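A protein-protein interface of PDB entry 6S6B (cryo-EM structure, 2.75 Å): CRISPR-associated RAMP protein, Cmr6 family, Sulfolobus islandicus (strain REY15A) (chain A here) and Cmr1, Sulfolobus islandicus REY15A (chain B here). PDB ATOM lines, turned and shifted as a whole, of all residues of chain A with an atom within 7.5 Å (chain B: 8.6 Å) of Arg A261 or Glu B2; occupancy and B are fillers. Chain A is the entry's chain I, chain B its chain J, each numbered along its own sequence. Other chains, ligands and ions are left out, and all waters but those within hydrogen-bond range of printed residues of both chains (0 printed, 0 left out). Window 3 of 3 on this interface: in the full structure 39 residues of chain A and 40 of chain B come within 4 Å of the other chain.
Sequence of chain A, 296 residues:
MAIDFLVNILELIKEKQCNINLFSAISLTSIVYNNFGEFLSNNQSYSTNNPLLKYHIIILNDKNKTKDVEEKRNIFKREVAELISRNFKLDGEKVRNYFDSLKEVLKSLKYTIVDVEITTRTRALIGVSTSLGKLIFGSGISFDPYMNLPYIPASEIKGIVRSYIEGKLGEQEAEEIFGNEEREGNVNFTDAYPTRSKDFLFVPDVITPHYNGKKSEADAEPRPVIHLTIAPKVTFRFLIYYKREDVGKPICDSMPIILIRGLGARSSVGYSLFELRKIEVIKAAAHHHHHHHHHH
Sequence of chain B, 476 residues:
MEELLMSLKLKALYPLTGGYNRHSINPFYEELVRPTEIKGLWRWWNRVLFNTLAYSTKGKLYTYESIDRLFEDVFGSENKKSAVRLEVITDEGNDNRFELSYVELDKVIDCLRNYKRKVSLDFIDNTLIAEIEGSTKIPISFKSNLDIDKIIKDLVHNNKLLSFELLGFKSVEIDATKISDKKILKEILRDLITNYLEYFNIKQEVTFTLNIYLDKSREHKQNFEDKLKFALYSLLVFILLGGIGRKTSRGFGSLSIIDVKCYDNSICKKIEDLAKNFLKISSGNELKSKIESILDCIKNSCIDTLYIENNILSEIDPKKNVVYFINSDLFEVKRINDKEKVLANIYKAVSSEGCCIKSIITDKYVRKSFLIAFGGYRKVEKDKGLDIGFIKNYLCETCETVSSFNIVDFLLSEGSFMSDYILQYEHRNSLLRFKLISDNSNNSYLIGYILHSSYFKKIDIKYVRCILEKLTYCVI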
ATOM      1  N   ARG A 121      24.759  34.703  37.295  1.00  0.00           N
ATOM      2  CA  ARG A 121      25.945  34.961  36.489  1.00  0.00           C
ATOM      3  C   ARG A 121      25.827  36.269  35.719  1.00  0.00           C
ATOM      4  O   ARG A 121      26.740  37.097  35.745  1.00  0.00           O
ATOM      5  CB  ARG A 121      26.183  33.808  35.516  1.00  0.00           C
ATOM      6  CG  ARG A 121      26.942  32.654  36.111  1.00  0.00           C
ATOM      7  CD  ARG A 121      27.082  31.549  35.097  1.00  0.00           C
ATOM      8  NE  ARG A 121      27.320  32.086  33.764  1.00  0.00           N
ATOM      9  CZ  ARG A 121      26.979  31.464  32.642  1.00  0.00           C
ATOM     10  NH1 ARG A 121      26.380  30.283  32.699  1.00  0.00           N
ATOM     11  NH2 ARG A 121      27.233  32.022  31.468  1.00  0.00           N
ATOM     12  N   ILE A 160      10.359  24.744  35.390  1.00  0.00           N
ATOM     13  CA  ILE A 160      11.530  24.701  34.524  1.00  0.00           C
ATOM     14  C   ILE A 160      12.204  23.343  34.611  1.00  0.00           C
ATOM     15  O   ILE A 160      12.577  22.752  33.594  1.00  0.00           O
ATOM     16  CB  ILE A 160      12.500  25.834  34.888  1.00  0.00           C
ATOM     17  CG1 ILE A 160      11.928  27.181  34.473  1.00  0.00           C
ATOM     18  CG2 ILE A 160      13.791  25.654  34.179  1.00  0.00           C
ATOM     19  CD1 ILE A 160      12.884  28.327  34.667  1.00  0.00           C
ATOM     20  N   SER A 163      10.134  20.704  32.725  1.00  0.00           N
ATOM     21  CA  SER A 163      10.263  20.751  31.275  1.00  0.00           C
ATOM     22  C   SER A 163      11.558  20.110  30.808  1.00  0.00           C
ATOM     23  O   SER A 163      11.639  19.631  29.673  1.00  0.00           O
ATOM     24  CB  SER A 163      10.188  22.190  30.780  1.00  0.00           C
ATOM     25  OG  SER A 163      11.431  22.837  30.952  1.00  0.00           O
ATOM     26  N   TYR A 164      12.582  20.089  31.661  1.00  0.00           N
ATOM     27  CA  TYR A 164      13.832  19.452  31.276  1.00  0.00           C
ATOM     28  C   TYR A 164      13.780  17.945  31.448  1.00  0.00           C
ATOM     29  O   TYR A 164      14.383  17.218  30.657  1.00  0.00           O
ATOM     30  CB  TYR A 164      14.996  20.012  32.082  1.00  0.00           C
ATOM     31  CG  TYR A 164      16.247  19.184  31.942  1.00  0.00           C
ATOM     32  CD1 TYR A 164      17.024  19.258  30.798  1.00  0.00           C
ATOM     33  CD2 TYR A 164      16.637  18.309  32.940  1.00  0.00           C
ATOM     34  CE1 TYR A 164      18.162  18.495  30.662  1.00  0.00           C
ATOM     35  CE2 TYR A 164      17.771  17.541  32.811  1.00  0.00           C
ATOM     36  CZ  TYR A 164      18.528  17.636  31.672  1.00  0.00           C
ATOM     37  OH  TYR A 164      19.660  16.868  31.549  1.00  0.00           O
ATOM     38  N   MET A 255      19.524  19.412  38.056  1.00  0.00           N
ATOM     39  CA  MET A 255      19.728  20.763  38.563  1.00  0.00           C
ATOM     40  C   MET A 255      20.900  21.474  37.890  1.00  0.00           C
ATOM     41  O   MET A 255      20.685  22.531  37.290  1.00  0.00           O
ATOM     42  CB  MET A 255      19.912  20.748  40.083  1.00  0.00           C
ATOM     43  CG  MET A 255      18.613  20.654  40.861  1.00  0.00           C
ATOM     44  SD  MET A 255      17.379  21.844  40.313  1.00  0.00           S
ATOM     45  CE  MET A 255      18.237  23.379  40.631  1.00  0.00           C
ATOM     46  N   PRO A 256      22.129  20.944  37.932  1.00  0.00           N
ATOM     47  CA  PRO A 256      23.255  21.713  37.378  1.00  0.00           C
ATOM     48  C   PRO A 256      23.090  22.079  35.917  1.00  0.00           C
ATOM     49  O   PRO A 256      23.510  23.167  35.510  1.00  0.00           O
ATOM     50  CB  PRO A 256      24.452  20.776  37.585  1.00  0.00           C
ATOM     51  CG  PRO A 256      23.864  19.437  37.713  1.00  0.00           C
ATOM     52  CD  PRO A 256      22.588  19.641  38.441  1.00  0.00           C
ATOM     53  N   ILE A 257      22.473  21.211  35.119  1.00  0.00           N
ATOM     54  CA  ILE A 257      22.319  21.485  33.694  1.00  0.00           C
ATOM     55  C   ILE A 257      21.325  22.615  33.471  1.00  0.00           C
ATOM     56  O   ILE A 257      21.553  23.513  32.654  1.00  0.00           O
ATOM     57  CB  ILE A 257      21.888  20.211  32.948  1.00  0.00           C
ATOM     58  CG1 ILE A 257      23.006  19.170  32.970  1.00  0.00           C
ATOM     59  CG2 ILE A 257      21.469  20.540  31.528  1.00  0.00           C
ATOM     60  CD1 ILE A 257      22.934  18.213  34.123  1.00  0.00           C
ATOM     61  N   ILE A 258      20.210  22.588  34.195  1.00  0.00           N
ATOM     62  CA  ILE A 258      19.110  23.488  33.884  1.00  0.00           C
ATOM     63  C   ILE A 258      19.463  24.930  34.221  1.00  0.00           C
ATOM     64  O   ILE A 258      18.961  25.864  33.584  1.00  0.00           O
ATOM     65  CB  ILE A 258      17.853  23.024  34.632  1.00  0.00           C
ATOM     66  CG1 ILE A 258      17.528  21.586  34.270  1.00  0.00           C
ATOM     67  CG2 ILE A 258      16.687  23.855  34.241  1.00  0.00           C
ATOM     68  CD1 ILE A 258      16.496  20.981  35.169  1.00  0.00           C
ATOM     69  N   LEU A 259      20.337  25.141  35.204  1.00  0.00           N
ATOM     70  CA  LEU A 259      20.664  26.498  35.625  1.00  0.00           C
ATOM     71  C   LEU A 259      21.498  27.229  34.585  1.00  0.00           C
ATOM     72  O   LEU A 259      21.325  28.435  34.386  1.00  0.00           O
ATOM     73  CB  LEU A 259      21.404  26.469  36.954  1.00  0.00           C
ATOM     74  CG  LEU A 259      20.814  25.498  37.961  1.00  0.00           C
ATOM     75  CD1 LEU A 259      21.787  25.262  39.088  1.00  0.00           C
ATOM     76  CD2 LEU A 259      19.500  26.025  38.480  1.00  0.00           C
ATOM     77  N   ILE A 260      22.426  26.527  33.929  1.00  0.00           N
ATOM     78  CA  ILE A 260      23.305  27.193  32.978  1.00  0.00           C
ATOM     79  C   ILE A 260      22.534  27.708  31.774  1.00  0.00           C
ATOM     80  O   ILE A 260      23.005  28.620  31.086  1.00  0.00           O
ATOM     81  CB  ILE A 260      24.443  26.254  32.540  1.00  0.00           C
ATOM     82  CG1 ILE A 260      23.950  25.252  31.499  1.00  0.00           C
ATOM     83  CG2 ILE A 260      25.011  25.519  33.736  1.00  0.00           C
ATOM     84  CD1 ILE A 260      25.054  24.441  30.873  1.00  0.00           C
ATOM     85  N   ARG A 261      21.366  27.146  31.494  1.00  0.00           N
ATOM     86  CA  ARG A 261      20.465  27.706  30.500  1.00  0.00           C
ATOM     87  C   ARG A 261      19.621  28.783  31.174  1.00  0.00           C
ATOM     88  O   ARG A 261      19.890  29.197  32.302  1.00  0.00           O
ATOM     89  CB  ARG A 261      19.628  26.600  29.872  1.00  0.00           C
ATOM     90  CG  ARG A 261      20.429  25.359  29.550  1.00  0.00           C
ATOM     91  CD  ARG A 261      19.558  24.271  28.966  1.00  0.00           C
ATOM     92  NE  ARG A 261      20.360  23.187  28.408  1.00  0.00           N
ATOM     93  CZ  ARG A 261      19.866  22.014  28.031  1.00  0.00           C
ATOM     94  NH1 ARG A 261      18.570  21.769  28.155  1.00  0.00           N
ATOM     95  NH2 ARG A 261      20.667  21.084  27.532  1.00  0.00           N
ATOM     96  N   GLY A 262      18.582  29.254  30.497  1.00  0.00           N
ATOM     97  CA  GLY A 262      17.779  30.326  31.057  1.00  0.00           C
ATOM     98  C   GLY A 262      16.989  29.872  32.272  1.00  0.00           C
ATOM     99  O   GLY A 262      16.511  28.740  32.343  1.00  0.00           O
ATOM    100  N   LEU A 263      16.865  30.772  33.243  1.00  0.00           N
ATOM    101  CA  LEU A 263      16.012  30.566  34.408  1.00  0.00           C
ATOM    102  C   LEU A 263      15.223  31.845  34.668  1.00  0.00           C
ATOM    103  O   LEU A 263      15.200  32.383  35.773  1.00  0.00           O
ATOM    104  CB  LEU A 263      16.831  30.149  35.628  1.00  0.00           C
ATOM    105  CG  LEU A 263      16.136  29.388  36.763  1.00  0.00           C
ATOM    106  CD1 LEU A 263      17.161  28.539  37.470  1.00  0.00           C
ATOM    107  CD2 LEU A 263      15.427  30.258  37.774  1.00  0.00           C
ATOM    108  N   GLY A 264      14.605  32.382  33.627  1.00  0.00           N
ATOM    109  CA  GLY A 264      13.838  33.603  33.799  1.00  0.00           C
ATOM    110  C   GLY A 264      13.439  34.184  32.467  1.00  0.00           C
ATOM    111  O   GLY A 264      13.261  33.459  31.485  1.00  0.00           O
ATOM    112  N   SER A 267      15.982  35.213  28.376  1.00  0.00           N
ATOM    113  CA  SER A 267      17.199  34.417  28.375  1.00  0.00           C
ATOM    114  C   SER A 267      17.640  34.018  26.979  1.00  0.00           C
ATOM    115  O   SER A 267      18.709  33.421  26.833  1.00  0.00           O
ATOM    116  CB  SER A 267      17.012  33.163  29.218  1.00  0.00           C
ATOM    117  OG  SER A 267      16.115  32.271  28.589  1.00  0.00           O
ATOM    118  N   SER A 272      19.178  35.825  32.143  1.00  0.00           N
ATOM    119  CA  SER A 272      19.024  35.132  33.415  1.00  0.00           C
ATOM    120  C   SER A 272      19.665  33.751  33.336  1.00  0.00           C
ATOM    121  O   SER A 272      19.005  32.721  33.225  1.00  0.00           O
ATOM    122  CB  SER A 272      17.554  35.057  33.801  1.00  0.00           C
ATOM    123  OG  SER A 272      16.840  34.250  32.892  1.00  0.00           O
ATOM    124  N   LEU A 273      20.989  33.753  33.409  1.00  0.00           N
ATOM    125  CA  LEU A 273      21.778  32.535  33.462  1.00  0.00           C
ATOM    126  C   LEU A 273      22.378  32.387  34.850  1.00  0.00           C
ATOM    127  O   LEU A 273      22.873  33.357  35.427  1.00  0.00           O
ATOM    128  CB  LEU A 273      22.879  32.550  32.406  1.00  0.00           C
ATOM    129  CG  LEU A 273      22.374  32.909  31.012  1.00  0.00           C
ATOM    130  CD1 LEU A 273      23.531  33.241  30.104  1.00  0.00           C
ATOM    131  CD2 LEU A 273      21.556  31.772  30.446  1.00  0.00           C
ATOM    132  N   PHE A 274      22.331  31.180  35.382  1.00  0.00           N
ATOM    133  CA  PHE A 274      22.674  30.944  36.773  1.00  0.00           C
ATOM    134  C   PHE A 274      23.870  30.006  36.863  1.00  0.00           C
ATOM    135  O   PHE A 274      24.495  29.659  35.860  1.00  0.00           O
ATOM    136  CB  PHE A 274      21.463  30.403  37.530  1.00  0.00           C
ATOM    137  CG  PHE A 274      20.492  31.464  37.940  1.00  0.00           C
ATOM    138  CD1 PHE A 274      19.649  32.037  37.017  1.00  0.00           C
ATOM    139  CD2 PHE A 274      20.430  31.893  39.247  1.00  0.00           C
ATOM    140  CE1 PHE A 274      18.761  33.014  37.390  1.00  0.00           C
ATOM    141  CE2 PHE A 274      19.545  32.866  39.622  1.00  0.00           C
ATOM    142  CZ  PHE A 274      18.710  33.428  38.693  1.00  0.00           C
ATOM    143  N   GLU A 275      24.185  29.594  38.086  1.00  0.00           N
ATOM    144  CA  GLU A 275      25.389  28.812  38.343  1.00  0.00           C
ATOM    145  C   GLU A 275      25.175  28.017  39.617  1.00  0.00           C
ATOM    146  O   GLU A 275      24.991  28.607  40.681  1.00  0.00           O
ATOM    147  CB  GLU A 275      26.590  29.730  38.483  1.00  0.00           C
ATOM    148  CG  GLU A 275      27.887  29.162  37.972  1.00  0.00           C
ATOM    149  CD  GLU A 275      28.992  30.192  37.986  1.00  0.00           C
ATOM    150  OE1 GLU A 275      29.234  30.784  39.058  1.00  0.00           O
ATOM    151  OE2 GLU A 275      29.613  30.415  36.927  1.00  0.00           O
ATOM    152  N   GLU B   2      18.829  21.022  23.596  1.00  0.00           N
ATOM    153  CA  GLU B   2      19.613  22.205  23.268  1.00  0.00           C
ATOM    154  C   GLU B   2      21.090  21.867  23.130  1.00  0.00           C
ATOM    155  O   GLU B   2      21.610  21.027  23.860  1.00  0.00           O
ATOM    156  CB  GLU B   2      19.415  23.284  24.330  1.00  0.00           C
ATOM    157  CG  GLU B   2      20.182  24.562  24.064  1.00  0.00           C
ATOM    158  CD  GLU B   2      19.794  25.682  25.001  1.00  0.00           C
ATOM    159  OE1 GLU B   2      18.894  25.478  25.838  1.00  0.00           O
ATOM    160  OE2 GLU B   2      20.396  26.769  24.902  1.00  0.00           O
ATOM    161  N   GLU B   3      21.767  22.519  22.188  1.00  0.00           N
ATOM    162  CA  GLU B   3      23.176  22.248  21.956  1.00  0.00           C
ATOM    163  C   GLU B   3      23.806  23.444  21.261  1.00  0.00           C
ATOM    164  O   GLU B   3      23.127  24.212  20.577  1.00  0.00           O
ATOM    165  CB  GLU B   3      23.362  20.972  21.129  1.00  0.00           C
ATOM    166  CG  GLU B   3      22.774  21.040  19.735  1.00  0.00           C
ATOM    167  CD  GLU B   3      23.776  21.511  18.700  1.00  0.00           C
ATOM    168  OE1 GLU B   3      24.991  21.380  18.949  1.00  0.00           O
ATOM    169  OE2 GLU B   3      23.351  22.015  17.640  1.00  0.00           O
ATOM    170  N   LEU B   4      25.114  23.587  21.449  1.00  0.00           N
ATOM    171  CA  LEU B   4      25.841  24.737  20.928  1.00  0.00           C
ATOM    172  C   LEU B   4      25.968  24.639  19.414  1.00  0.00           C
ATOM    173  O   LEU B   4      26.541  23.679  18.892  1.00  0.00           O
ATOM    174  CB  LEU B   4      27.218  24.812  21.576  1.00  0.00           C
ATOM    175  CG  LEU B   4      28.178  25.877  21.062  1.00  0.00           C
ATOM    176  CD1 LEU B   4      27.525  27.239  21.093  1.00  0.00           C
ATOM    177  CD2 LEU B   4      29.438  25.875  21.898  1.00  0.00           C
ATOM    178  N   LEU B   5      25.451  25.643  18.708  1.00  0.00           N
ATOM    179  CA  LEU B   5      25.492  25.616  17.251  1.00  0.00           C
ATOM    180  C   LEU B   5      26.868  26.002  16.727  1.00  0.00           C
ATOM    181  O   LEU B   5      27.481  25.252  15.962  1.00  0.00           O
ATOM    182  CB  LEU B   5      24.424  26.543  16.677  1.00  0.00           C
ATOM    183  CG  LEU B   5      24.050  26.299  15.221  1.00  0.00           C
ATOM    184  CD1 LEU B   5      23.588  24.870  15.042  1.00  0.00           C
ATOM    185  CD2 LEU B   5      22.975  27.265  14.783  1.00  0.00           C
ATOM    186  N   LYS B  81       8.943  31.413  21.057  1.00  0.00           N
ATOM    187  CA  LYS B  81      10.241  31.754  21.613  1.00  0.00           C
ATOM    188  C   LYS B  81      11.309  31.640  20.535  1.00  0.00           C
ATOM    189  O   LYS B  81      11.139  30.941  19.534  1.00  0.00           O
ATOM    190  CB  LYS B  81      10.564  30.829  22.783  1.00  0.00           C
ATOM    191  CG  LYS B  81      11.779  31.215  23.595  1.00  0.00           C
ATOM    192  CD  LYS B  81      12.230  30.053  24.445  1.00  0.00           C
ATOM    193  CE  LYS B  81      13.048  30.514  25.623  1.00  0.00           C
ATOM    194  NZ  LYS B  81      14.202  31.314  25.163  1.00  0.00           N
ATOM    195  N   SER B  82      12.417  32.342  20.735  1.00  0.00           N
ATOM    196  CA  SER B  82      13.516  32.257  19.788  1.00  0.00           C
ATOM    197  C   SER B  82      14.091  30.848  19.761  1.00  0.00           C
ATOM    198  O   SER B  82      14.170  30.163  20.783  1.00  0.00           O
ATOM    199  CB  SER B  82      14.609  33.254  20.146  1.00  0.00           C
ATOM    200  OG  SER B  82      15.698  33.149  19.253  1.00  0.00           O
ATOM    201  N   ALA B  83      14.497  30.417  18.570  1.00  0.00           N
ATOM    202  CA  ALA B  83      15.139  29.121  18.413  1.00  0.00           C
ATOM    203  C   ALA B  83      16.632  29.192  18.659  1.00  0.00           C
ATOM    204  O   ALA B  83      17.215  28.234  19.175  1.00  0.00           O
ATOM    205  CB  ALA B  83      14.880  28.568  17.013  1.00  0.00           C
ATOM    206  N   VAL B  84      17.259  30.298  18.297  1.00  0.00           N
ATOM    207  CA  VAL B  84      18.652  30.559  18.622  1.00  0.00           C
ATOM    208  C   VAL B  84      18.687  31.454  19.846  1.00  0.00           C
ATOM    209  O   VAL B  84      17.848  32.347  20.001  1.00  0.00           O
ATOM    210  CB  VAL B  84      19.392  31.208  17.439  1.00  0.00           C
ATOM    211  CG1 VAL B  84      19.463  30.248  16.274  1.00  0.00           C
ATOM    212  CG2 VAL B  84      18.703  32.497  17.021  1.00  0.00           C
ATOM    213  N   ARG B  85      19.647  31.209  20.731  1.00  0.00           N
ATOM    214  CA  ARG B  85      19.857  32.075  21.881  1.00  0.00           C
ATOM    215  C   ARG B  85      21.323  32.454  21.937  1.00  0.00           C
ATOM    216  O   ARG B  85      22.197  31.583  21.940  1.00  0.00           O
ATOM    217  CB  ARG B  85      19.409  31.411  23.184  1.00  0.00           C
ATOM    218  CG  ARG B  85      20.050  30.091  23.520  1.00  0.00           C
ATOM    219  CD  ARG B  85      19.886  29.824  24.999  1.00  0.00           C
ATOM    220  NE  ARG B  85      20.760  30.675  25.795  1.00  0.00           N
ATOM    221  CZ  ARG B  85      21.872  30.255  26.384  1.00  0.00           C
ATOM    222  NH1 ARG B  85      22.239  28.988  26.284  1.00  0.00           N
ATOM    223  NH2 ARG B  85      22.611  31.099  27.085  1.00  0.00           N
ATOM    224  N   LEU B  86      21.589  33.753  21.960  1.00  0.00           N
ATOM    225  CA  LEU B  86      22.952  34.241  21.972  1.00  0.00           C
ATOM    226  C   LEU B  86      23.519  34.209  23.383  1.00  0.00           C
ATOM    227  O   LEU B  86      22.795  34.261  24.378  1.00  0.00           O
ATOM    228  CB  LEU B  86      23.019  35.664  21.432  1.00  0.00           C
ATOM    229  CG  LEU B  86      22.215  35.911  20.166  1.00  0.00           C
ATOM    230  CD1 LEU B  86      22.453  37.317  19.686  1.00  0.00           C
ATOM    231  CD2 LEU B  86      22.596  34.913  19.107  1.00  0.00           C
ATOM    232  N   GLU B  87      24.839  34.124  23.458  1.00  0.00           N
ATOM    233  CA  GLU B  87      25.529  34.259  24.731  1.00  0.00           C
ATOM    234  C   GLU B  87      26.879  34.891  24.460  1.00  0.00           C
ATOM    235  O   GLU B  87      27.769  34.239  23.913  1.00  0.00           O
ATOM    236  CB  GLU B  87      25.700  32.911  25.425  1.00  0.00           C
ATOM    237  CG  GLU B  87      26.348  33.024  26.787  1.00  0.00           C
ATOM    238  CD  GLU B  87      26.494  31.687  27.474  1.00  0.00           C
ATOM    239  OE1 GLU B  87      26.122  30.666  26.859  1.00  0.00           O
ATOM    240  OE2 GLU B  87      26.975  31.655  28.626  1.00  0.00           O
ATOM    241  N   ILE B 212      26.342  30.736  19.976  1.00  0.00           N
ATOM    242  CA  ILE B 212      24.981  30.678  19.467  1.00  0.00           C
ATOM    243  C   ILE B 212      24.479  29.261  19.658  1.00  0.00           C
ATOM    244  O   ILE B 212      25.100  28.311  19.172  1.00  0.00           O
ATOM    245  CB  ILE B 212      24.906  31.092  17.993  1.00  0.00           C
ATOM    246  CG1 ILE B 212      25.268  32.566  17.859  1.00  0.00           C
ATOM    247  CG2 ILE B 212      23.528  30.817  17.432  1.00  0.00           C
ATOM    248  CD1 ILE B 212      25.124  33.093  16.473  1.00  0.00           C
ATOM    249  N   TYR B 213      23.370  29.115  20.371  1.00  0.00           N
ATOM    250  CA  TYR B 213      22.839  27.808  20.712  1.00  0.00           C
ATOM    251  C   TYR B 213      21.594  27.519  19.893  1.00  0.00           C
ATOM    252  O   TYR B 213      20.875  28.430  19.481  1.00  0.00           O
ATOM    253  CB  TYR B 213      22.501  27.718  22.199  1.00  0.00           C
ATOM    254  CG  TYR B 213      23.694  27.850  23.110  1.00  0.00           C
ATOM    255  CD1 TYR B 213      24.281  29.081  23.336  1.00  0.00           C
ATOM    256  CD2 TYR B 213      24.228  26.744  23.746  1.00  0.00           C
ATOM    257  CE1 TYR B 213      25.364  29.209  24.164  1.00  0.00           C
ATOM    258  CE2 TYR B 213      25.313  26.863  24.577  1.00  0.00           C
ATOM    259  CZ  TYR B 213      25.878  28.099  24.783  1.00  0.00           C
ATOM    260  OH  TYR B 213      26.965  28.228  25.613  1.00  0.00           O
ATOM    261  N   LEU B 214      21.356  26.237  19.653  1.00  0.00           N
ATOM    262  CA  LEU B 214      20.119  25.762  19.065  1.00  0.00           C
ATOM    263  C   LEU B 214      19.438  24.834  20.057  1.00  0.00           C
ATOM    264  O   LEU B 214      20.082  24.248  20.928  1.00  0.00           O
ATOM    265  CB  LEU B 214      20.363  25.032  17.744  1.00  0.00           C
ATOM    266  CG  LEU B 214      19.241  25.191  16.724  1.00  0.00           C
ATOM    267  CD1 LEU B 214      19.124  26.633  16.288  1.00  0.00           C
ATOM    268  CD2 LEU B 214      19.476  24.286  15.536  1.00  0.00           C
ATOM    269  N   ASP B 215      18.123  24.701  19.918  1.00  0.00           N
ATOM    270  CA  ASP B 215      17.337  23.949  20.883  1.00  0.00           C
ATOM    271  C   ASP B 215      17.068  22.511  20.467  1.00  0.00           C
ATOM    272  O   ASP B 215      16.717  21.694  21.326  1.00  0.00           O
ATOM    273  CB  ASP B 215      15.999  24.645  21.121  1.00  0.00           C
ATOM    274  CG  ASP B 215      15.071  24.503  19.945  1.00  0.00           C
ATOM    275  OD1 ASP B 215      15.569  24.529  18.801  1.00  0.00           O
ATOM    276  OD2 ASP B 215      13.850  24.361  20.165  1.00  0.00           O
ATOM    277  N   LYS B 216      17.208  22.185  19.181  1.00  0.00           N
ATOM    278  CA  LYS B 216      16.932  20.853  18.647  1.00  0.00           C
ATOM    279  C   LYS B 216      15.506  20.396  18.933  1.00  0.00           C
ATOM    280  O   LYS B 216      15.217  19.196  18.898  1.00  0.00           O
ATOM    281  CB  LYS B 216      17.927  19.817  19.179  1.00  0.00           C
ATOM    282  CG  LYS B 216      19.383  20.228  19.077  1.00  0.00           C
ATOM    283  CD  LYS B 216      19.744  20.677  17.670  1.00  0.00           C
ATOM    284  CE  LYS B 216      19.761  19.513  16.697  1.00  0.00           C
ATOM    285  NZ  LYS B 216      19.967  19.971  15.298  1.00  0.00           N
ATOM    286  N   SER B 217      14.607  21.335  19.227  1.00  0.00           N
ATOM    287  CA  SER B 217      13.203  21.030  19.464  1.00  0.00           C
ATOM    288  C   SER B 217      12.294  21.735  18.472  1.00  0.00           C
ATOM    289  O   SER B 217      11.067  21.694  18.628  1.00  0.00           O
ATOM    290  CB  SER B 217      12.805  21.406  20.892  1.00  0.00           C
ATOM    291  OG  SER B 217      11.420  21.194  21.102  1.00  0.00           O
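The guanidinium group (NH2) of Arg B85 lies within salt-bridge range of the side-chain carboxylate (OE1) of Glu B87 (3.5 Å).
The backbone NH (N) of Arg A121 is in hydrogen-bond range of the backbone carbonyl oxygen (O) of Leu A273, at 3.0 Å.
The side-chain carboxylate (OE2) of Glu B2 lies within salt-bridge range of the guanidinium group (NH1) of Arg B85 (3.2 Å).
The backbone NH of Glu B2 is in hydrogen-bond range of the backbone carbonyl oxygen of Asp B215 (3.2 Å).
O of Arg B85 lies within hydrogen-bond range of N of Tyr B213 (3.2 Å).
The side-chain carboxylate (OE1) of Glu B87 is in hydrogen-bond range of the side-chain hydroxyl (OH) of Tyr B213 (2.9 Å).
The guanidinium group (NH2) of Arg A121 is in salt-bridge range of the side-chain carboxylate (OE2) of Glu B87 (2.9 Å).
The side-chain carboxylate (OE1) of Glu B2 lies within salt-bridge range of the guanidinium group (NE) of Arg A261 (3.7 Å).
Of the 17 printed residues of chain B, 3 touch a printed residue of chain A.
Of the 19 printed residues of chain A, 4 touch a printed residue of chain B.
Printed residues of chain A that touch a printed residue of chain B: Arg A121, Arg A261, Ser A267 and Leu A273.
Hydrophobic or aromatic side chains of chain A within 4 Å of the printed part of chain B: Leu A273.
Among the printed residues, 4 pairs touch across the chains.
Among the printed residues, Asp or Glu carboxylates within 4 Å of a Lys or Arg side-chain nitrogen of the other chain: Arg A121 with Glu B87 (2.9 Å) and Arg A261 with Glu B2 (3.7 Å).
O of Ser A267 touches NE of Arg B85 (3.6 Å).
Arg B85 touches Leu A273 (NH2 to CD2, 3.6 Å).
Of the printed residues of chain A, Glu B2 touches Arg A261 (3.4 Å).
Of the printed residues of chain B, Ser A267 touches Arg B85 (3.6 Å).
Printed residues of chain A within 4 Å of Arg B85: Ser A267 and Leu A273.
Printed residues of chain B within 4 Å of Leu A273: Arg B85.
Of the printed residues of chain A, Glu B87 touches Arg A121 (2.9 Å).
Met A255 touches none of the printed residues of chain B.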
